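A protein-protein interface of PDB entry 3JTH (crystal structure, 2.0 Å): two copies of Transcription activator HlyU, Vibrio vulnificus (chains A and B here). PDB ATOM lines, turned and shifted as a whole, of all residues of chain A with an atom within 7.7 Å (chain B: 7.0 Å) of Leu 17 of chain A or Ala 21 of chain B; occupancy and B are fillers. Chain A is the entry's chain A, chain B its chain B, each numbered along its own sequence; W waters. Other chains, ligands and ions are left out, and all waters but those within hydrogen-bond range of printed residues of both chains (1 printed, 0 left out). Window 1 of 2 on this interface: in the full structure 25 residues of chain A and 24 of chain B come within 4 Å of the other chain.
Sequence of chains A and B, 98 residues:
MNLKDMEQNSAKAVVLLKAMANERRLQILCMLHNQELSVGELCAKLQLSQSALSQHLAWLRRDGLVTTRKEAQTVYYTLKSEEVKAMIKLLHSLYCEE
Printed residues of chain B that touch a printed residue of chain A: Leu 17, Lys 18, Met 20, Ala 21, Asn 22, Glu 23, Leu 26, Met 87, Leu 91 and Tyr 95.
Hydrophobic or aromatic side chains of chain B within 4 Å of the printed part of chain A: Leu 17, Met 20, Ala 21, Leu 26, Met 87, Leu 91 and Tyr 95.
Of the 17 printed residues of chain A, 11 touch a printed residue of chain B.
Printed residues of chain A that touch a printed residue of chain B: Ser 10, Ala 11, Lys 12, Ala 13, Val 14, Leu 16, Leu 17, Lys 18, Met 20, Ala 21 and Met 87.
Among the printed residues, no Asp or Glu carboxylate lies within 4 Å of a Lys or Arg side-chain nitrogen of the other chain.
Among the printed residues, pairs that only touch across the chains: Ser 10 of chain A with Leu 26 of chain B, Ala 11 of chain A with Glu 23 of chain B, Lys 12 of chain A with Tyr 95 of chain B, Ala 13 of chain A with Leu 26 of chain B, Ala 13 of chain A with Tyr 95 of chain B, Val 14 of chain A with Ala 21 of chain B, Val 14 of chain A with Asn 22 of chain B, Val 14 of chain A with Glu 23 of chain B, Leu 16 of chain A with Tyr 95 of chain B, Leu 17 of chain A with Met 20 of chain B, Leu 17 of chain A with Ala 21 of chain B, Lys 18 of chain A with Ala 21 of chain B, Met 20 of chain A with Leu 17 of chain B, Ala 21 of chain A with Leu 17 of chain B, Ala 21 of chain A with Lys 18 of chain B, Met 87 of chain A with Met 87 of chain B and Met 87 of chain A with Leu 91 of chain B.
The backbone carbonyl oxygen (O) of Lys 18 of chain A is in hydrogen-bond range of the guanidinium group (NH2) of Arg 25 of chain A, 3.4 Å away.
The guanidinium group of Arg 25 of chain B is in hydrogen-bond range of the backbone carbonyl oxygen of Lys 18 of chain B (3.0 Å).
OD1 of Asn 22 of chain B sits at hydrogen-bond distance from N of Arg 24 of chain B, at 3.1 Å.
The side-chain amide oxygen of Asn 22 of chain B sits at hydrogen-bond distance from the backbone NH of Arg 25 of chain B (3.1 Å).
Leu 17 of chain A touches just these residues of chain B: Met 20 (3.5 Å) and Ala 21 (3.9 Å).
Of chain A, only Val 14, Leu 17 and Lys 18 come within 4 Å of Ala 21 of chain B.
Printed residues of chain A within 4 Å of Lys 18 of chain B: Ala 21 (3.4 Å).
Of the printed residues of chain B, Leu 16 of chain A touches Tyr 95 (3.9 Å).
Printed residues of chain B within 4 Å of Met 20 of chain A: Leu 17.
Printed residues of chain B within 4 Å of Val 14 of chain A: Ala 21, Asn 22 and Glu 23.
Val 15 of chain A touches none of the printed residues of chain B.
Arg 25 of chain A touches none of the printed residues of chain B.
The nearest residue of chain A that does not touch Ala 21 of chain B is Ala 21 of chain A (5.1 Å).
Water W1 bridges O of Ala 11 of chain A (2.5 Å) and OE1 of Glu 23 of chain B (2.5 Å).
Leu 17 of chain A touches Met 20 of chain B, and with the chains exchanged Met 20 of chain A touches Leu 17 of chain B.
Leu 17 of chain A touches Ala 21 of chain B, and with the chains exchanged Ala 21 of chain A touches Leu 17 of chain B.
Lys 18 of chain A touches Ala 21 of chain B, and with the chains exchanged Ala 21 of chain A touches Lys 18 of chain B.
Met 87 of chain B touches its own counterpart, Met 87 of chain A.
Positions printed for both chains: 16, 17, 18, 19, 20, 21, 22, 25 and 87.
Of the 17 pairs that touch across the chains among the printed residues, 7 have their exchanged pair printed and touching as well.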
ATOM      1  N   SER A  10      -7.929   4.410 -27.673  1.00  0.00           N
ATOM      2  CA  SER A  10      -8.665   4.410 -26.415  1.00  0.00           C
ATOM      3  C   SER A  10      -7.909   5.356 -25.480  1.00  0.00           C
ATOM      4  O   SER A  10      -8.512   6.075 -24.680  1.00  0.00           O
ATOM      5  CB  SER A  10      -8.716   3.000 -25.809  1.00  0.00           C
ATOM      6  OG  SER A  10      -7.442   2.574 -25.355  1.00  0.00           O
ATOM      7  N   ALA A  11      -6.584   5.361 -25.597  1.00  0.00           N
ATOM      8  CA  ALA A  11      -5.759   6.234 -24.775  1.00  0.00           C
ATOM      9  C   ALA A  11      -6.016   7.707 -25.119  1.00  0.00           C
ATOM     10  O   ALA A  11      -6.135   8.540 -24.227  1.00  0.00           O
ATOM     11  CB  ALA A  11      -4.274   5.894 -24.964  1.00  0.00           C
ATOM     12  N   LYS A  12      -6.111   8.024 -26.409  1.00  0.00           N
ATOM     13  CA  LYS A  12      -6.353   9.403 -26.843  1.00  0.00           C
ATOM     14  C   LYS A  12      -7.739   9.854 -26.388  1.00  0.00           C
ATOM     15  O   LYS A  12      -7.929  10.992 -25.958  1.00  0.00           O
ATOM     16  CB  LYS A  12      -6.246   9.511 -28.368  1.00  0.00           C
ATOM     17  CG  LYS A  12      -4.849   9.233 -28.884  1.00  0.00           C
ATOM     18  CD  LYS A  12      -4.854   8.683 -30.291  1.00  0.00           C
ATOM     19  CE  LYS A  12      -3.438   8.204 -30.637  1.00  0.00           C
ATOM     20  NZ  LYS A  12      -3.373   7.192 -31.739  1.00  0.00           N
ATOM     21  N   ALA A  13      -8.704   8.951 -26.483  1.00  0.00           N
ATOM     22  CA  ALA A  13     -10.059   9.254 -26.061  1.00  0.00           C
ATOM     23  C   ALA A  13     -10.078   9.532 -24.559  1.00  0.00           C
ATOM     24  O   ALA A  13     -10.676  10.510 -24.114  1.00  0.00           O
ATOM     25  CB  ALA A  13     -10.978   8.087 -26.394  1.00  0.00           C
ATOM     26  N   VAL A  14      -9.419   8.681 -23.776  1.00  0.00           N
ATOM     27  CA  VAL A  14      -9.390   8.871 -22.326  1.00  0.00           C
ATOM     28  C   VAL A  14      -8.763  10.206 -21.951  1.00  0.00           C
ATOM     29  O   VAL A  14      -9.098  10.784 -20.916  1.00  0.00           O
ATOM     30  CB  VAL A  14      -8.625   7.735 -21.625  1.00  0.00           C
ATOM     31  CG1 VAL A  14      -8.422   8.073 -20.160  1.00  0.00           C
ATOM     32  CG2 VAL A  14      -9.404   6.430 -21.765  1.00  0.00           C
ATOM     33  N   VAL A  15      -7.857  10.699 -22.791  1.00  0.00           N
ATOM     34  CA  VAL A  15      -7.217  11.993 -22.547  1.00  0.00           C
ATOM     35  C   VAL A  15      -8.287  13.092 -22.539  1.00  0.00           C
ATOM     36  O   VAL A  15      -8.393  13.869 -21.595  1.00  0.00           O
ATOM     37  CB  VAL A  15      -6.174  12.316 -23.641  1.00  0.00           C
ATOM     38  CG1 VAL A  15      -5.841  13.810 -23.634  1.00  0.00           C
ATOM     39  CG2 VAL A  15      -4.910  11.486 -23.400  1.00  0.00           C
ATOM     40  N   LEU A  16      -9.074  13.151 -23.604  1.00  0.00           N
ATOM     41  CA  LEU A  16     -10.140  14.143 -23.703  1.00  0.00           C
ATOM     42  C   LEU A  16     -11.146  13.928 -22.568  1.00  0.00           C
ATOM     43  O   LEU A  16     -11.565  14.879 -21.906  1.00  0.00           O
ATOM     44  CB  LEU A  16     -10.855  14.005 -25.053  1.00  0.00           C
ATOM     45  CG  LEU A  16     -12.079  14.885 -25.318  1.00  0.00           C
ATOM     46  CD1 LEU A  16     -11.671  16.353 -25.365  1.00  0.00           C
ATOM     47  CD2 LEU A  16     -12.712  14.475 -26.631  1.00  0.00           C
ATOM     48  N   LEU A  17     -11.529  12.675 -22.351  1.00  0.00           N
ATOM     49  CA  LEU A  17     -12.506  12.330 -21.315  1.00  0.00           C
ATOM     50  C   LEU A  17     -12.159  12.855 -19.927  1.00  0.00           C
ATOM     51  O   LEU A  17     -13.001  13.434 -19.247  1.00  0.00           O
ATOM     52  CB  LEU A  17     -12.692  10.814 -21.273  1.00  0.00           C
ATOM     53  CG  LEU A  17     -13.923  10.201 -21.948  1.00  0.00           C
ATOM     54  CD1 LEU A  17     -14.401  11.053 -23.106  1.00  0.00           C
ATOM     55  CD2 LEU A  17     -13.570   8.795 -22.404  1.00  0.00           C
ATOM     56  N   LYS A  18     -10.914  12.644 -19.511  1.00  0.00           N
ATOM     57  CA  LYS A  18     -10.448  13.108 -18.214  1.00  0.00           C
ATOM     58  C   LYS A  18     -10.463  14.623 -18.138  1.00  0.00           C
ATOM     59  O   LYS A  18     -10.779  15.198 -17.100  1.00  0.00           O
ATOM     60  CB  LYS A  18      -9.024  12.609 -17.947  1.00  0.00           C
ATOM     61  CG  LYS A  18      -8.931  11.140 -17.572  1.00  0.00           C
ATOM     62  CD  LYS A  18      -7.484  10.713 -17.352  1.00  0.00           C
ATOM     63  CE  LYS A  18      -7.399   9.247 -16.939  1.00  0.00           C
ATOM     64  NZ  LYS A  18      -5.996   8.807 -16.713  1.00  0.00           N
ATOM     65  N   ALA A  19     -10.109  15.272 -19.237  1.00  0.00           N
ATOM     66  CA  ALA A  19     -10.090  16.728 -19.260  1.00  0.00           C
ATOM     67  C   ALA A  19     -11.493  17.285 -19.072  1.00  0.00           C
ATOM     68  O   ALA A  19     -11.669  18.337 -18.464  1.00  0.00           O
ATOM     69  CB  ALA A  19      -9.516  17.228 -20.570  1.00  0.00           C
ATOM     70  N   MET A  20     -12.492  16.565 -19.578  1.00  0.00           N
ATOM     71  CA  MET A  20     -13.880  17.006 -19.492  1.00  0.00           C
ATOM     72  C   MET A  20     -14.626  16.584 -18.229  1.00  0.00           C
ATOM     73  O   MET A  20     -15.571  17.253 -17.808  1.00  0.00           O
ATOM     74  CB  MET A  20     -14.656  16.495 -20.708  1.00  0.00           C
ATOM     75  CG  MET A  20     -14.207  17.073 -22.040  1.00  0.00           C
ATOM     76  SD  MET A  20     -15.130  16.218 -23.524  1.00  0.00           S
ATOM     77  CE  MET A  20     -16.865  17.063 -23.274  1.00  0.00           C
ATOM     78  N   ALA A  21     -14.201  15.487 -17.616  1.00  0.00           N
ATOM     79  CA  ALA A  21     -14.886  14.959 -16.441  1.00  0.00           C
ATOM     80  C   ALA A  21     -14.747  15.740 -15.130  1.00  0.00           C
ATOM     81  O   ALA A  21     -14.168  15.255 -14.164  1.00  0.00           O
ATOM     82  CB  ALA A  21     -14.469  13.503 -16.224  1.00  0.00           C
ATOM     83  N   ASN A  22     -15.306  16.941 -15.105  1.00  0.00           N
ATOM     84  CA  ASN A  22     -15.316  17.798 -13.925  1.00  0.00           C
ATOM     85  C   ASN A  22     -16.504  18.752 -14.093  1.00  0.00           C
ATOM     86  O   ASN A  22     -16.648  19.399 -15.122  1.00  0.00           O
ATOM     87  CB  ASN A  22     -14.019  18.607 -13.804  1.00  0.00           C
ATOM     88  CG  ASN A  22     -14.093  19.655 -12.701  1.00  0.00           C
ATOM     89  OD1 ASN A  22     -13.831  19.365 -11.532  1.00  0.00           O
ATOM     90  ND2 ASN A  22     -14.473  20.870 -13.065  1.00  0.00           N
ATOM     91  N   ARG A  25     -15.718  22.526 -15.143  1.00  0.00           N
ATOM     92  CA  ARG A  25     -15.110  22.619 -16.457  1.00  0.00           C
ATOM     93  C   ARG A  25     -16.143  22.315 -17.548  1.00  0.00           C
ATOM     94  O   ARG A  25     -16.206  23.010 -18.565  1.00  0.00           O
ATOM     95  CB  ARG A  25     -13.944  21.643 -16.591  1.00  0.00           C
ATOM     96  CG  ARG A  25     -12.762  21.979 -15.690  1.00  0.00           C
ATOM     97  CD  ARG A  25     -11.495  21.271 -16.173  1.00  0.00           C
ATOM     98  NE  ARG A  25     -11.566  19.820 -16.038  1.00  0.00           N
ATOM     99  CZ  ARG A  25     -11.041  19.136 -15.025  1.00  0.00           C
ATOM    100  NH1 ARG A  25     -10.404  19.771 -14.050  1.00  0.00           N
ATOM    101  NH2 ARG A  25     -11.137  17.813 -14.996  1.00  0.00           N
ATOM    102  N   ASP A  63      -4.884  22.283 -21.020  1.00  0.00           N
ATOM    103  CA  ASP A  63      -5.231  21.075 -21.760  1.00  0.00           C
ATOM    104  C   ASP A  63      -5.648  21.434 -23.193  1.00  0.00           C
ATOM    105  O   ASP A  63      -6.105  20.577 -23.944  1.00  0.00           O
ATOM    106  CB  ASP A  63      -6.368  20.329 -21.056  1.00  0.00           C
ATOM    107  CG  ASP A  63      -6.225  18.818 -21.159  1.00  0.00           C
ATOM    108  OD1 ASP A  63      -5.441  18.239 -20.374  1.00  0.00           O
ATOM    109  OD2 ASP A  63      -6.884  18.209 -22.031  1.00  0.00           O
ATOM    110  N   LEU A  65      -8.209  23.037 -24.411  1.00  0.00           N
ATOM    111  CA  LEU A  65      -9.616  22.844 -24.763  1.00  0.00           C
ATOM    112  C   LEU A  65     -10.331  24.170 -25.023  1.00  0.00           C
ATOM    113  O   LEU A  65     -11.432  24.195 -25.573  1.00  0.00           O
ATOM    114  CB  LEU A  65     -10.350  22.070 -23.659  1.00  0.00           C
ATOM    115  CG  LEU A  65      -9.996  20.587 -23.481  1.00  0.00           C
ATOM    116  CD1 LEU A  65     -10.879  19.972 -22.408  1.00  0.00           C
ATOM    117  CD2 LEU A  65     -10.179  19.846 -24.799  1.00  0.00           C
ATOM    118  N   MET A  87     -17.865  16.533 -28.901  1.00  0.00           N
ATOM    119  CA  MET A  87     -18.412  15.901 -27.702  1.00  0.00           C
ATOM    120  C   MET A  87     -19.368  16.874 -27.021  1.00  0.00           C
ATOM    121  O   MET A  87     -20.425  16.476 -26.530  1.00  0.00           O
ATOM    122  CB  MET A  87     -17.294  15.518 -26.727  1.00  0.00           C
ATOM    123  CG  MET A  87     -16.614  14.186 -27.029  1.00  0.00           C
ATOM    124  SD  MET A  87     -17.787  12.636 -26.863  1.00  0.00           S
ATOM    125  CE  MET A  87     -19.019  13.305 -25.529  1.00  0.00           C
ATOM    126  N   LEU B  16     -20.979  10.026 -16.135  1.00  0.00           N
ATOM    127  CA  LEU B  16     -20.810   9.127 -17.278  1.00  0.00           C
ATOM    128  C   LEU B  16     -19.379   9.252 -17.798  1.00  0.00           C
ATOM    129  O   LEU B  16     -18.719   8.256 -18.115  1.00  0.00           O
ATOM    130  CB  LEU B  16     -21.795   9.500 -18.390  1.00  0.00           C
ATOM    131  CG  LEU B  16     -23.048   8.646 -18.606  1.00  0.00           C
ATOM    132  CD1 LEU B  16     -23.579   8.085 -17.286  1.00  0.00           C
ATOM    133  CD2 LEU B  16     -24.096   9.499 -19.313  1.00  0.00           C
ATOM    134  N   LEU B  17     -18.902  10.490 -17.876  1.00  0.00           N
ATOM    135  CA  LEU B  17     -17.555  10.758 -18.368  1.00  0.00           C
ATOM    136  C   LEU B  17     -16.510  10.100 -17.493  1.00  0.00           C
ATOM    137  O   LEU B  17     -15.528   9.561 -18.001  1.00  0.00           O
ATOM    138  CB  LEU B  17     -17.307  12.268 -18.444  1.00  0.00           C
ATOM    139  CG  LEU B  17     -18.223  13.026 -19.415  1.00  0.00           C
ATOM    140  CD1 LEU B  17     -17.988  14.516 -19.284  1.00  0.00           C
ATOM    141  CD2 LEU B  17     -17.955  12.558 -20.851  1.00  0.00           C
ATOM    142  N   LYS B  18     -16.721  10.143 -16.180  1.00  0.00           N
ATOM    143  CA  LYS B  18     -15.791   9.531 -15.232  1.00  0.00           C
ATOM    144  C   LYS B  18     -15.743   8.014 -15.405  1.00  0.00           C
ATOM    145  O   LYS B  18     -14.676   7.418 -15.360  1.00  0.00           O
ATOM    146  CB  LYS B  18     -16.185   9.868 -13.797  1.00  0.00           C
ATOM    147  CG  LYS B  18     -16.091  11.342 -13.457  1.00  0.00           C
ATOM    148  CD  LYS B  18     -15.194  11.593 -12.258  1.00  0.00           C
ATOM    149  CE  LYS B  18     -15.257  13.050 -11.828  1.00  0.00           C
ATOM    150  NZ  LYS B  18     -14.378  13.329 -10.656  1.00  0.00           N
ATOM    151  N   ALA B  19     -16.899   7.389 -15.601  1.00  0.00           N
ATOM    152  CA  ALA B  19     -16.951   5.939 -15.795  1.00  0.00           C
ATOM    153  C   ALA B  19     -16.252   5.527 -17.106  1.00  0.00           C
ATOM    154  O   ALA B  19     -15.715   4.428 -17.227  1.00  0.00           O
ATOM    155  CB  ALA B  19     -18.403   5.480 -15.806  1.00  0.00           C
ATOM    156  N   MET B  20     -16.238   6.423 -18.081  1.00  0.00           N
ATOM    157  CA  MET B  20     -15.616   6.128 -19.367  1.00  0.00           C
ATOM    158  C   MET B  20     -14.132   6.490 -19.442  1.00  0.00           C
ATOM    159  O   MET B  20     -13.407   5.970 -20.297  1.00  0.00           O
ATOM    160  CB  MET B  20     -16.352   6.875 -20.485  1.00  0.00           C
ATOM    161  CG  MET B  20     -17.844   6.612 -20.578  1.00  0.00           C
ATOM    162  SD  MET B  20     -18.662   7.794 -21.931  1.00  0.00           S
ATOM    163  CE  MET B  20     -17.986   6.877 -23.520  1.00  0.00           C
ATOM    164  N   ALA B  21     -13.693   7.370 -18.544  1.00  0.00           N
ATOM    165  CA  ALA B  21     -12.315   7.868 -18.529  1.00  0.00           C
ATOM    166  C   ALA B  21     -11.252   6.934 -17.967  1.00  0.00           C
ATOM    167  O   ALA B  21     -10.517   7.285 -17.043  1.00  0.00           O
ATOM    168  CB  ALA B  21     -12.258   9.226 -17.789  1.00  0.00           C
ATOM    169  N   ASN B  22     -11.175   5.745 -18.541  1.00  0.00           N
ATOM    170  CA  ASN B  22     -10.200   4.743 -18.156  1.00  0.00           C
ATOM    171  C   ASN B  22     -10.066   3.843 -19.370  1.00  0.00           C
ATOM    172  O   ASN B  22     -11.049   3.285 -19.843  1.00  0.00           O
ATOM    173  CB  ASN B  22     -10.679   3.949 -16.937  1.00  0.00           C
ATOM    174  CG  ASN B  22      -9.774   2.780 -16.618  1.00  0.00           C
ATOM    175  OD1 ASN B  22      -9.842   1.734 -17.263  1.00  0.00           O
ATOM    176  ND2 ASN B  22      -8.915   2.952 -15.624  1.00  0.00           N
ATOM    177  N   GLU B  23      -8.850   3.699 -19.881  1.00  0.00           N
ATOM    178  CA  GLU B  23      -8.616   2.888 -21.071  1.00  0.00           C
ATOM    179  C   GLU B  23      -9.342   1.545 -21.111  1.00  0.00           C
ATOM    180  O   GLU B  23     -10.116   1.276 -22.034  1.00  0.00           O
ATOM    181  CB  GLU B  23      -7.115   2.674 -21.274  1.00  0.00           C
ATOM    182  CG  GLU B  23      -6.330   3.942 -21.624  1.00  0.00           C
ATOM    183  CD  GLU B  23      -6.056   4.826 -20.419  1.00  0.00           C
ATOM    184  OE1 GLU B  23      -5.429   5.888 -20.599  1.00  0.00           O
ATOM    185  OE2 GLU B  23      -6.459   4.461 -19.292  1.00  0.00           O
ATOM    186  N   ARG B  24      -9.098   0.702 -20.115  1.00  0.00           N
ATOM    187  CA  ARG B  24      -9.732  -0.604 -20.078  1.00  0.00           C
ATOM    188  C   ARG B  24     -11.266  -0.540 -20.050  1.00  0.00           C
ATOM    189  O   ARG B  24     -11.937  -1.271 -20.780  1.00  0.00           O
ATOM    190  CB  ARG B  24      -9.215  -1.397 -18.876  1.00  0.00           C
ATOM    191  CG  ARG B  24      -8.959  -2.858 -19.188  1.00  0.00           C
ATOM    192  CD  ARG B  24      -7.548  -3.106 -19.714  1.00  0.00           C
ATOM    193  NE  ARG B  24      -7.112  -2.095 -20.674  1.00  0.00           N
ATOM    194  CZ  ARG B  24      -6.108  -2.265 -21.530  1.00  0.00           C
ATOM    195  NH1 ARG B  24      -5.437  -3.410 -21.551  1.00  0.00           N
ATOM    196  NH2 ARG B  24      -5.768  -1.285 -22.360  1.00  0.00           N
ATOM    197  N   ARG B  25     -11.826   0.326 -19.214  1.00  0.00           N
ATOM    198  CA  ARG B  25     -13.279   0.439 -19.133  1.00  0.00           C
ATOM    199  C   ARG B  25     -13.895   0.906 -20.457  1.00  0.00           C
ATOM    200  O   ARG B  25     -14.984   0.470 -20.848  1.00  0.00           O
ATOM    201  CB  ARG B  25     -13.667   1.396 -18.001  1.00  0.00           C
ATOM    202  CG  ARG B  25     -13.281   0.885 -16.612  1.00  0.00           C
ATOM    203  CD  ARG B  25     -14.167   1.469 -15.523  1.00  0.00           C
ATOM    204  NE  ARG B  25     -14.080   2.919 -15.410  1.00  0.00           N
ATOM    205  CZ  ARG B  25     -13.249   3.564 -14.598  1.00  0.00           C
ATOM    206  NH1 ARG B  25     -12.421   2.886 -13.817  1.00  0.00           N
ATOM    207  NH2 ARG B  25     -13.267   4.893 -14.551  1.00  0.00           N
ATOM    208  N   LEU B  26     -13.181   1.783 -21.154  1.00  0.00           N
ATOM    209  CA  LEU B  26     -13.650   2.300 -22.433  1.00  0.00           C
ATOM    210  C   LEU B  26     -13.650   1.201 -23.480  1.00  0.00           C
ATOM    211  O   LEU B  26     -14.624   1.047 -24.203  1.00  0.00           O
ATOM    212  CB  LEU B  26     -12.781   3.474 -22.894  1.00  0.00           C
ATOM    213  CG  LEU B  26     -13.293   4.229 -24.129  1.00  0.00           C
ATOM    214  CD1 LEU B  26     -14.731   4.701 -23.907  1.00  0.00           C
ATOM    215  CD2 LEU B  26     -12.362   5.402 -24.418  1.00  0.00           C
ATOM    216  N   LEU B  29     -16.650  -0.989 -22.926  1.00  0.00           N
ATOM    217  CA  LEU B  29     -17.838  -0.273 -23.395  1.00  0.00           C
ATOM    218  C   LEU B  29     -17.867  -0.250 -24.923  1.00  0.00           C
ATOM    219  O   LEU B  29     -18.926  -0.399 -25.540  1.00  0.00           O
ATOM    220  CB  LEU B  29     -17.837   1.166 -22.863  1.00  0.00           C
ATOM    221  CG  LEU B  29     -18.025   1.326 -21.348  1.00  0.00           C
ATOM    222  CD1 LEU B  29     -17.701   2.759 -20.932  1.00  0.00           C
ATOM    223  CD2 LEU B  29     -19.462   0.937 -20.967  1.00  0.00           C
ATOM    224  N   MET B  87     -22.204   8.513 -27.002  1.00  0.00           N
ATOM    225  CA  MET B  87     -20.824   8.976 -26.861  1.00  0.00           C
ATOM    226  C   MET B  87     -19.817   7.990 -27.440  1.00  0.00           C
ATOM    227  O   MET B  87     -18.810   8.399 -28.012  1.00  0.00           O
ATOM    228  CB  MET B  87     -20.499   9.252 -25.390  1.00  0.00           C
ATOM    229  CG  MET B  87     -21.116  10.542 -24.893  1.00  0.00           C
ATOM    230  SD  MET B  87     -20.839  10.842 -23.016  1.00  0.00           S
ATOM    231  CE  MET B  87     -22.503  10.124 -22.345  1.00  0.00           C
ATOM    232  N   LEU B  91     -17.120   8.796 -30.260  1.00  0.00           N
ATOM    233  CA  LEU B  91     -15.713   8.499 -30.002  1.00  0.00           C
ATOM    234  C   LEU B  91     -15.176   7.640 -31.151  1.00  0.00           C
ATOM    235  O   LEU B  91     -14.096   7.900 -31.679  1.00  0.00           O
ATOM    236  CB  LEU B  91     -15.566   7.756 -28.672  1.00  0.00           C
ATOM    237  CG  LEU B  91     -15.087   8.508 -27.418  1.00  0.00           C
ATOM    238  CD1 LEU B  91     -15.081  10.015 -27.636  1.00  0.00           C
ATOM    239  CD2 LEU B  91     -15.981   8.127 -26.242  1.00  0.00           C
ATOM    240  N   TYR B  95     -11.918   8.838 -33.488  1.00  0.00           N
ATOM    241  CA  TYR B  95     -10.622   8.162 -33.454  1.00  0.00           C
ATOM    242  C   TYR B  95     -10.561   6.901 -34.314  1.00  0.00           C
ATOM    243  O   TYR B  95      -9.758   6.004 -34.059  1.00  0.00           O
ATOM    244  CB  TYR B  95     -10.255   7.827 -32.006  1.00  0.00           C
ATOM    245  CG  TYR B  95     -10.200   9.049 -31.113  1.00  0.00           C
ATOM    246  CD1 TYR B  95      -9.179   9.993 -31.249  1.00  0.00           C
ATOM    247  CD2 TYR B  95     -11.205   9.300 -30.178  1.00  0.00           C
ATOM    248  CE1 TYR B  95      -9.166  11.159 -30.482  1.00  0.00           C
ATOM    249  CE2 TYR B  95     -11.205  10.462 -29.409  1.00  0.00           C
ATOM    250  CZ  TYR B  95     -10.186  11.388 -29.566  1.00  0.00           C
ATOM    251  OH  TYR B  95     -10.200  12.548 -28.822  1.00  0.00           O
HETATM  252  O   HOH W   1      -4.935   7.834 -22.144  1.00  0.00           O
